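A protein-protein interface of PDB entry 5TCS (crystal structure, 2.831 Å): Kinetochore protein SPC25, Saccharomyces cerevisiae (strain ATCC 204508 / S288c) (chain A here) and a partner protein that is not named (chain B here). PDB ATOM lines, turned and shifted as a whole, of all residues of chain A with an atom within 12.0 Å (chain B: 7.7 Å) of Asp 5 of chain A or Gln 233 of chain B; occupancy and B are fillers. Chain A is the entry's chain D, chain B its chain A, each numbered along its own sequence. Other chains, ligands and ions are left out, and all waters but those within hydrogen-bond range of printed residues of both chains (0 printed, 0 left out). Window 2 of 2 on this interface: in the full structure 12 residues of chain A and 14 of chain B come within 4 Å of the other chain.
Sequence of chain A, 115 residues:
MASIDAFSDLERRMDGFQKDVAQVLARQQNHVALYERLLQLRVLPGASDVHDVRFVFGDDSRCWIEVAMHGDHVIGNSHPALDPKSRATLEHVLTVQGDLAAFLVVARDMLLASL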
ATOM      1  N   ALA A   2     -21.138 -21.575  -5.473  1.00  0.00           N
ATOM      2  CA  ALA A   2     -20.505 -20.682  -4.510  1.00  0.00           C
ATOM      3  C   ALA A   2     -20.836 -19.228  -4.826  1.00  0.00           C
ATOM      4  O   ALA A   2     -19.948 -18.377  -4.886  1.00  0.00           O
ATOM      5  CB  ALA A   2     -19.002 -20.895  -4.500  1.00  0.00           C
ATOM      6  N   SER A   3     -22.121 -18.952  -5.030  1.00  0.00           N
ATOM      7  CA  SER A   3     -22.611 -17.610  -5.308  1.00  0.00           C
ATOM      8  C   SER A   3     -23.365 -17.079  -4.096  1.00  0.00           C
ATOM      9  O   SER A   3     -24.034 -17.839  -3.387  1.00  0.00           O
ATOM     10  CB  SER A   3     -23.524 -17.606  -6.538  1.00  0.00           C
ATOM     11  OG  SER A   3     -24.215 -16.374  -6.661  1.00  0.00           O
ATOM     12  N   ILE A   4     -23.253 -15.769  -3.860  1.00  0.00           N
ATOM     13  CA  ILE A   4     -23.919 -15.161  -2.712  1.00  0.00           C
ATOM     14  C   ILE A   4     -25.416 -15.436  -2.750  1.00  0.00           C
ATOM     15  O   ILE A   4     -26.067 -15.520  -1.701  1.00  0.00           O
ATOM     16  CB  ILE A   4     -23.617 -13.649  -2.663  1.00  0.00           C
ATOM     17  CG1 ILE A   4     -23.827 -13.109  -1.247  1.00  0.00           C
ATOM     18  CG2 ILE A   4     -24.486 -12.885  -3.663  1.00  0.00           C
ATOM     19  CD1 ILE A   4     -23.305 -11.700  -1.044  1.00  0.00           C
ATOM     20  N   ASP A   5     -25.987 -15.579  -3.948  1.00  0.00           N
ATOM     21  CA  ASP A   5     -27.401 -15.920  -4.055  1.00  0.00           C
ATOM     22  C   ASP A   5     -27.704 -17.256  -3.389  1.00  0.00           C
ATOM     23  O   ASP A   5     -28.830 -17.480  -2.932  1.00  0.00           O
ATOM     24  CB  ASP A   5     -27.823 -15.953  -5.524  1.00  0.00           C
ATOM     25  CG  ASP A   5     -27.813 -14.579  -6.167  1.00  0.00           C
ATOM     26  OD1 ASP A   5     -27.994 -13.580  -5.439  1.00  0.00           O
ATOM     27  OD2 ASP A   5     -27.626 -14.498  -7.399  1.00  0.00           O
ATOM     28  N   ALA A   6     -26.720 -18.150  -3.327  1.00  0.00           N
ATOM     29  CA  ALA A   6     -26.885 -19.445  -2.680  1.00  0.00           C
ATOM     30  C   ALA A   6     -26.672 -19.384  -1.172  1.00  0.00           C
ATOM     31  O   ALA A   6     -26.652 -20.436  -0.522  1.00  0.00           O
ATOM     32  CB  ALA A   6     -25.922 -20.463  -3.294  1.00  0.00           C
ATOM     33  N   PHE A   7     -26.519 -18.185  -0.604  1.00  0.00           N
ATOM     34  CA  PHE A   7     -26.263 -18.078   0.829  1.00  0.00           C
ATOM     35  C   PHE A   7     -27.372 -18.725   1.643  1.00  0.00           C
ATOM     36  O   PHE A   7     -27.112 -19.266   2.723  1.00  0.00           O
ATOM     37  CB  PHE A   7     -26.105 -16.614   1.230  1.00  0.00           C
ATOM     38  CG  PHE A   7     -25.715 -16.426   2.663  1.00  0.00           C
ATOM     39  CD1 PHE A   7     -24.518 -16.937   3.135  1.00  0.00           C
ATOM     40  CD2 PHE A   7     -26.541 -15.743   3.540  1.00  0.00           C
ATOM     41  CE1 PHE A   7     -24.151 -16.773   4.453  1.00  0.00           C
ATOM     42  CE2 PHE A   7     -26.177 -15.574   4.859  1.00  0.00           C
ATOM     43  CZ  PHE A   7     -24.978 -16.090   5.315  1.00  0.00           C
ATOM     44  N   SER A   8     -28.612 -18.670   1.149  1.00  0.00           N
ATOM     45  CA  SER A   8     -29.700 -19.404   1.784  1.00  0.00           C
ATOM     46  C   SER A   8     -29.234 -20.798   2.184  1.00  0.00           C
ATOM     47  O   SER A   8     -29.311 -21.180   3.357  1.00  0.00           O
ATOM     48  CB  SER A   8     -30.895 -19.480   0.833  1.00  0.00           C
ATOM     49  OG  SER A   8     -30.492 -19.914  -0.455  1.00  0.00           O
ATOM     50  N   ASP A   9     -28.702 -21.553   1.219  1.00  0.00           N
ATOM     51  CA  ASP A   9     -28.249 -22.912   1.492  1.00  0.00           C
ATOM     52  C   ASP A   9     -27.351 -22.955   2.718  1.00  0.00           C
ATOM     53  O   ASP A   9     -27.557 -23.768   3.626  1.00  0.00           O
ATOM     54  CB  ASP A   9     -27.515 -23.475   0.272  1.00  0.00           C
ATOM     55  CG  ASP A   9     -28.435 -23.697  -0.914  1.00  0.00           C
ATOM     56  OD1 ASP A   9     -29.671 -23.661  -0.727  1.00  0.00           O
ATOM     57  OD2 ASP A   9     -27.924 -23.915  -2.033  1.00  0.00           O
ATOM     58  N   LEU A  10     -26.347 -22.079   2.772  1.00  0.00           N
ATOM     59  CA  LEU A  10     -25.417 -22.125   3.893  1.00  0.00           C
ATOM     60  C   LEU A  10     -26.141 -21.878   5.210  1.00  0.00           C
ATOM     61  O   LEU A  10     -25.880 -22.563   6.207  1.00  0.00           O
ATOM     62  CB  LEU A  10     -24.289 -21.112   3.688  1.00  0.00           C
ATOM     63  CG  LEU A  10     -22.996 -21.382   4.469  1.00  0.00           C
ATOM     64  CD1 LEU A  10     -22.401 -22.747   4.127  1.00  0.00           C
ATOM     65  CD2 LEU A  10     -21.974 -20.287   4.202  1.00  0.00           C
ATOM     66  N   GLU A  11     -27.086 -20.932   5.225  1.00  0.00           N
ATOM     67  CA  GLU A  11     -27.828 -20.663   6.453  1.00  0.00           C
ATOM     68  C   GLU A  11     -28.461 -21.931   7.004  1.00  0.00           C
ATOM     69  O   GLU A  11     -28.654 -22.050   8.219  1.00  0.00           O
ATOM     70  CB  GLU A  11     -28.906 -19.603   6.214  1.00  0.00           C
ATOM     71  CG  GLU A  11     -28.367 -18.232   5.837  1.00  0.00           C
ATOM     72  CD  GLU A  11     -29.324 -17.112   6.199  1.00  0.00           C
ATOM     73  OE1 GLU A  11     -29.412 -16.770   7.397  1.00  0.00           O
ATOM     74  OE2 GLU A  11     -29.995 -16.582   5.288  1.00  0.00           O
ATOM     75  N   ARG A  12     -28.790 -22.892   6.137  1.00  0.00           N
ATOM     76  CA  ARG A  12     -29.266 -24.181   6.617  1.00  0.00           C
ATOM     77  C   ARG A  12     -28.177 -24.849   7.442  1.00  0.00           C
ATOM     78  O   ARG A  12     -28.331 -25.028   8.655  1.00  0.00           O
ATOM     79  CB  ARG A  12     -29.689 -25.081   5.451  1.00  0.00           C
ATOM     80  CG  ARG A  12     -31.168 -25.003   5.096  1.00  0.00           C
ATOM     81  CD  ARG A  12     -31.441 -25.560   3.700  1.00  0.00           C
ATOM     82  NE  ARG A  12     -31.749 -26.989   3.707  1.00  0.00           N
ATOM     83  CZ  ARG A  12     -31.820 -27.744   2.615  1.00  0.00           C
ATOM     84  NH1 ARG A  12     -31.593 -27.214   1.419  1.00  0.00           N
ATOM     85  NH2 ARG A  12     -32.110 -29.034   2.714  1.00  0.00           N
ATOM     86  N   MET A  14     -25.390 -23.964   8.751  1.00  0.00           N
ATOM     87  CA  MET A  14     -25.023 -23.218   9.946  1.00  0.00           C
ATOM     88  C   MET A  14     -26.063 -23.427  11.041  1.00  0.00           C
ATOM     89  O   MET A  14     -25.719 -23.815  12.159  1.00  0.00           O
ATOM     90  CB  MET A  14     -24.863 -21.733   9.617  1.00  0.00           C
ATOM     91  CG  MET A  14     -23.517 -21.417   8.982  1.00  0.00           C
ATOM     92  SD  MET A  14     -23.459 -19.744   7.994  1.00  0.00           S
ATOM     93  CE  MET A  14     -23.093 -18.519   9.447  1.00  0.00           C
ATOM     94  N   LYS B 226     -29.875  -2.799  -8.707  1.00  0.00           N
ATOM     95  CA  LYS B 226     -29.179  -4.054  -8.445  1.00  0.00           C
ATOM     96  C   LYS B 226     -28.121  -3.873  -7.363  1.00  0.00           C
ATOM     97  O   LYS B 226     -28.062  -4.650  -6.402  1.00  0.00           O
ATOM     98  CB  LYS B 226     -28.550  -4.587  -9.733  1.00  0.00           C
ATOM     99  CG  LYS B 226     -29.538  -4.810 -10.873  1.00  0.00           C
ATOM    100  CD  LYS B 226     -29.234  -6.100 -11.638  1.00  0.00           C
ATOM    101  CE  LYS B 226     -29.253  -5.914 -13.151  1.00  0.00           C
ATOM    102  NZ  LYS B 226     -30.574  -6.242 -13.756  1.00  0.00           N
ATOM    103  N   ARG B 227     -27.277  -2.850  -7.507  1.00  0.00           N
ATOM    104  CA  ARG B 227     -26.247  -2.562  -6.515  1.00  0.00           C
ATOM    105  C   ARG B 227     -26.815  -2.609  -5.103  1.00  0.00           C
ATOM    106  O   ARG B 227     -26.351  -3.382  -4.257  1.00  0.00           O
ATOM    107  CB  ARG B 227     -25.629  -1.194  -6.806  1.00  0.00           C
ATOM    108  CG  ARG B 227     -24.560  -0.757  -5.815  1.00  0.00           C
ATOM    109  CD  ARG B 227     -23.343  -0.233  -6.549  1.00  0.00           C
ATOM    110  NE  ARG B 227     -23.715   0.743  -7.574  1.00  0.00           N
ATOM    111  CZ  ARG B 227     -23.170   0.827  -8.785  1.00  0.00           C
ATOM    112  NH1 ARG B 227     -22.217  -0.017  -9.161  1.00  0.00           N
ATOM    113  NH2 ARG B 227     -23.588   1.757  -9.632  1.00  0.00           N
ATOM    114  N   TYR B 228     -27.824  -1.780  -4.831  1.00  0.00           N
ATOM    115  CA  TYR B 228     -28.507  -1.841  -3.545  1.00  0.00           C
ATOM    116  C   TYR B 228     -28.885  -3.279  -3.214  1.00  0.00           C
ATOM    117  O   TYR B 228     -28.439  -3.841  -2.206  1.00  0.00           O
ATOM    118  CB  TYR B 228     -29.747  -0.943  -3.568  1.00  0.00           C
ATOM    119  CG  TYR B 228     -30.552  -0.987  -2.289  1.00  0.00           C
ATOM    120  CD1 TYR B 228     -30.214  -0.183  -1.206  1.00  0.00           C
ATOM    121  CD2 TYR B 228     -31.646  -1.832  -2.160  1.00  0.00           C
ATOM    122  CE1 TYR B 228     -30.942  -0.222  -0.032  1.00  0.00           C
ATOM    123  CE2 TYR B 228     -32.382  -1.877  -0.990  1.00  0.00           C
ATOM    124  CZ  TYR B 228     -32.025  -1.069   0.071  1.00  0.00           C
ATOM    125  OH  TYR B 228     -32.752  -1.107   1.240  1.00  0.00           O
ATOM    126  N   LYS B 229     -29.687  -3.900  -4.084  1.00  0.00           N
ATOM    127  CA  LYS B 229     -30.091  -5.289  -3.883  1.00  0.00           C
ATOM    128  C   LYS B 229     -28.902  -6.155  -3.492  1.00  0.00           C
ATOM    129  O   LYS B 229     -29.010  -7.014  -2.610  1.00  0.00           O
ATOM    130  CB  LYS B 229     -30.739  -5.829  -5.158  1.00  0.00           C
ATOM    131  CG  LYS B 229     -31.879  -6.809  -4.930  1.00  0.00           C
ATOM    132  CD  LYS B 229     -33.167  -6.088  -4.554  1.00  0.00           C
ATOM    133  CE  LYS B 229     -34.387  -6.974  -4.754  1.00  0.00           C
ATOM    134  NZ  LYS B 229     -34.629  -7.282  -6.196  1.00  0.00           N
ATOM    135  N   LEU B 230     -27.753  -5.934  -4.134  1.00  0.00           N
ATOM    136  CA  LEU B 230     -26.574  -6.736  -3.834  1.00  0.00           C
ATOM    137  C   LEU B 230     -26.023  -6.404  -2.456  1.00  0.00           C
ATOM    138  O   LEU B 230     -25.799  -7.300  -1.635  1.00  0.00           O
ATOM    139  CB  LEU B 230     -25.503  -6.517  -4.904  1.00  0.00           C
ATOM    140  CG  LEU B 230     -24.211  -7.315  -4.715  1.00  0.00           C
ATOM    141  CD1 LEU B 230     -24.490  -8.812  -4.732  1.00  0.00           C
ATOM    142  CD2 LEU B 230     -23.197  -6.947  -5.784  1.00  0.00           C
ATOM    143  N   HIS B 231     -25.793  -5.119  -2.182  1.00  0.00           N
ATOM    144  CA  HIS B 231     -25.188  -4.749  -0.908  1.00  0.00           C
ATOM    145  C   HIS B 231     -26.000  -5.305   0.253  1.00  0.00           C
ATOM    146  O   HIS B 231     -25.444  -5.897   1.187  1.00  0.00           O
ATOM    147  CB  HIS B 231     -25.051  -3.230  -0.814  1.00  0.00           C
ATOM    148  CG  HIS B 231     -23.920  -2.681  -1.626  1.00  0.00           C
ATOM    149  ND1 HIS B 231     -23.385  -1.428  -1.411  1.00  0.00           N
ATOM    150  CD2 HIS B 231     -23.218  -3.218  -2.653  1.00  0.00           C
ATOM    151  CE1 HIS B 231     -22.404  -1.218  -2.271  1.00  0.00           C
ATOM    152  NE2 HIS B 231     -22.282  -2.287  -3.037  1.00  0.00           N
ATOM    153  N   GLN B 232     -27.325  -5.152   0.195  1.00  0.00           N
ATOM    154  CA  GLN B 232     -28.191  -5.769   1.192  1.00  0.00           C
ATOM    155  C   GLN B 232     -27.786  -7.220   1.428  1.00  0.00           C
ATOM    156  O   GLN B 232     -27.439  -7.608   2.550  1.00  0.00           O
ATOM    157  CB  GLN B 232     -29.652  -5.676   0.744  1.00  0.00           C
ATOM    158  CG  GLN B 232     -30.161  -4.251   0.565  1.00  0.00           C
ATOM    159  CD  GLN B 232     -30.098  -3.437   1.843  1.00  0.00           C
ATOM    160  OE1 GLN B 232     -29.388  -2.433   1.921  1.00  0.00           O
ATOM    161  NE2 GLN B 232     -30.847  -3.861   2.853  1.00  0.00           N
ATOM    162  N   GLN B 233     -27.796  -8.031   0.365  1.00  0.00           N
ATOM    163  CA  GLN B 233     -27.351  -9.416   0.466  1.00  0.00           C
ATOM    164  C   GLN B 233     -26.060  -9.517   1.269  1.00  0.00           C
ATOM    165  O   GLN B 233     -25.996 -10.228   2.279  1.00  0.00           O
ATOM    166  CB  GLN B 233     -27.156 -10.020  -0.930  1.00  0.00           C
ATOM    167  CG  GLN B 233     -28.441 -10.321  -1.678  1.00  0.00           C
ATOM    168  CD  GLN B 233     -28.181 -10.971  -3.024  1.00  0.00           C
ATOM    169  OE1 GLN B 233     -27.513 -10.397  -3.886  1.00  0.00           O
ATOM    170  NE2 GLN B 233     -28.697 -12.181  -3.206  1.00  0.00           N
ATOM    171  N   VAL B 234     -25.023  -8.790   0.841  1.00  0.00           N
ATOM    172  CA  VAL B 234     -23.751  -8.807   1.561  1.00  0.00           C
ATOM    173  C   VAL B 234     -23.998  -8.542   3.041  1.00  0.00           C
ATOM    174  O   VAL B 234     -23.664  -9.358   3.905  1.00  0.00           O
ATOM    175  CB  VAL B 234     -22.774  -7.784   0.956  1.00  0.00           C
ATOM    176  CG1 VAL B 234     -21.692  -7.386   1.958  1.00  0.00           C
ATOM    177  CG2 VAL B 234     -22.135  -8.365  -0.294  1.00  0.00           C
ATOM    178  N   ILE B 235     -24.619  -7.408   3.348  1.00  0.00           N
ATOM    179  CA  ILE B 235     -24.963  -7.034   4.717  1.00  0.00           C
ATOM    180  C   ILE B 235     -25.562  -8.266   5.387  1.00  0.00           C
ATOM    181  O   ILE B 235     -25.066  -8.722   6.427  1.00  0.00           O
ATOM    182  CB  ILE B 235     -25.936  -5.835   4.752  1.00  0.00           C
ATOM    183  CG1 ILE B 235     -25.165  -4.542   4.486  1.00  0.00           C
ATOM    184  CG2 ILE B 235     -26.661  -5.750   6.092  1.00  0.00           C
ATOM    185  CD1 ILE B 235     -25.983  -3.466   3.816  1.00  0.00           C
ATOM    186  N   HIS B 236     -26.608  -8.819   4.772  1.00  0.00           N
ATOM    187  CA  HIS B 236     -27.287  -9.970   5.351  1.00  0.00           C
ATOM    188  C   HIS B 236     -26.279 -11.010   5.828  1.00  0.00           C
ATOM    189  O   HIS B 236     -26.258 -11.370   7.010  1.00  0.00           O
ATOM    190  CB  HIS B 236     -28.260 -10.580   4.340  1.00  0.00           C
ATOM    191  CG  HIS B 236     -29.087 -11.701   4.890  1.00  0.00           C
ATOM    192  ND1 HIS B 236     -29.716 -11.633   6.115  1.00  0.00           N
ATOM    193  CD2 HIS B 236     -29.386 -12.921   4.381  1.00  0.00           C
ATOM    194  CE1 HIS B 236     -30.368 -12.762   6.336  1.00  0.00           C
ATOM    195  NE2 HIS B 236     -30.184 -13.560   5.300  1.00  0.00           N
ATOM    196  N   VAL B 237     -25.409 -11.481   4.929  1.00  0.00           N
ATOM    197  CA  VAL B 237     -24.460 -12.516   5.333  1.00  0.00           C
ATOM    198  C   VAL B 237     -23.612 -12.006   6.493  1.00  0.00           C
ATOM    199  O   VAL B 237     -23.569 -12.617   7.573  1.00  0.00           O
ATOM    200  CB  VAL B 237     -23.596 -12.996   4.143  1.00  0.00           C
ATOM    201  CG1 VAL B 237     -24.381 -12.992   2.821  1.00  0.00           C
ATOM    202  CG2 VAL B 237     -22.283 -12.217   3.992  1.00  0.00           C
ATOM    203  N   ILE B 238     -22.999 -10.829   6.320  1.00  0.00           N
ATOM    204  CA  ILE B 238     -22.131 -10.279   7.356  1.00  0.00           C
ATOM    205  C   ILE B 238     -22.872 -10.208   8.675  1.00  0.00           C
ATOM    206  O   ILE B 238     -22.264 -10.311   9.747  1.00  0.00           O
ATOM    207  CB  ILE B 238     -21.587  -8.896   6.932  1.00  0.00           C
ATOM    208  CG1 ILE B 238     -20.578  -9.065   5.790  1.00  0.00           C
ATOM    209  CG2 ILE B 238     -20.958  -8.169   8.130  1.00  0.00           C
ATOM    210  CD1 ILE B 238     -19.844  -7.792   5.388  1.00  0.00           C
ATOM    211  N   ASP B 239     -24.191 -10.041   8.628  1.00  0.00           N
ATOM    212  CA  ASP B 239     -24.961 -10.067   9.858  1.00  0.00           C
ATOM    213  C   ASP B 239     -24.936 -11.476  10.429  1.00  0.00           C
ATOM    214  O   ASP B 239     -24.280 -11.729  11.445  1.00  0.00           O
ATOM    215  CB  ASP B 239     -26.399  -9.601   9.624  1.00  0.00           C
ATOM    216  CG  ASP B 239     -27.242  -9.662  10.885  1.00  0.00           C
ATOM    217  OD1 ASP B 239     -26.672  -9.544  11.991  1.00  0.00           O
ATOM    218  OD2 ASP B 239     -28.473  -9.832  10.768  1.00  0.00           O
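OD1 of Asp 5 of chain A lies within hydrogen-bond range of NE2 of Gln 233 of chain B (2.7 Å). A ring nitrogen (NE2) of His 236 of chain B sits at hydrogen-bond distance from the side-chain carboxylate (OE2) of Glu 11 of chain A (3.0 Å).
OG of Ser 3 of chain A sits close to N of Asp 5 of chain A (3.3 Å).
Among the printed residues, merely in contact across the chains: Phe 7 of chain A with Val 237 of chain B, Ile 4 of chain A with Val 234 of chain B and Ile 4 of chain A with Gln 233 of chain B.
Of the printed residues of chain B, Ile 4 of chain A touches Gln 233 and Val 234. Of chain B, only Gln 233 (2.7 Å) comes within 4 Å of Asp 5 of chain A. Of the printed residues of chain B, Phe 7 of chain A touches Val 237 (3.5 Å). Of the printed residues of chain B, Glu 11 of chain A touches His 236 (3.0 Å). Arg 12 of chain A touches none of the printed residues of chain B. Lys 226 of chain B touches none of the printed residues of chain A. Gln 232 of chain B touches none of the printed residues of chain A. Of chain A, only Ile 4 (3.9 Å) and Asp 5 (2.7 Å) come within 4 Å of Gln 233 of chain B. Of chain A, only Glu 11 comes within 4 Å of His 236 of chain B.
Of the 14 printed residues of chain B, 4 touch a printed residue of chain A. Hydrophobic or aromatic side chains of chain B that line the printed part of chain A: Val 234, His 236 and Val 237. Of the 12 printed residues of chain A, 4 touch a printed residue of chain B. Hydrophobic or aromatic side chains of chain A within 4 Å of the printed part of chain B: Ile 4 and Phe 7.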
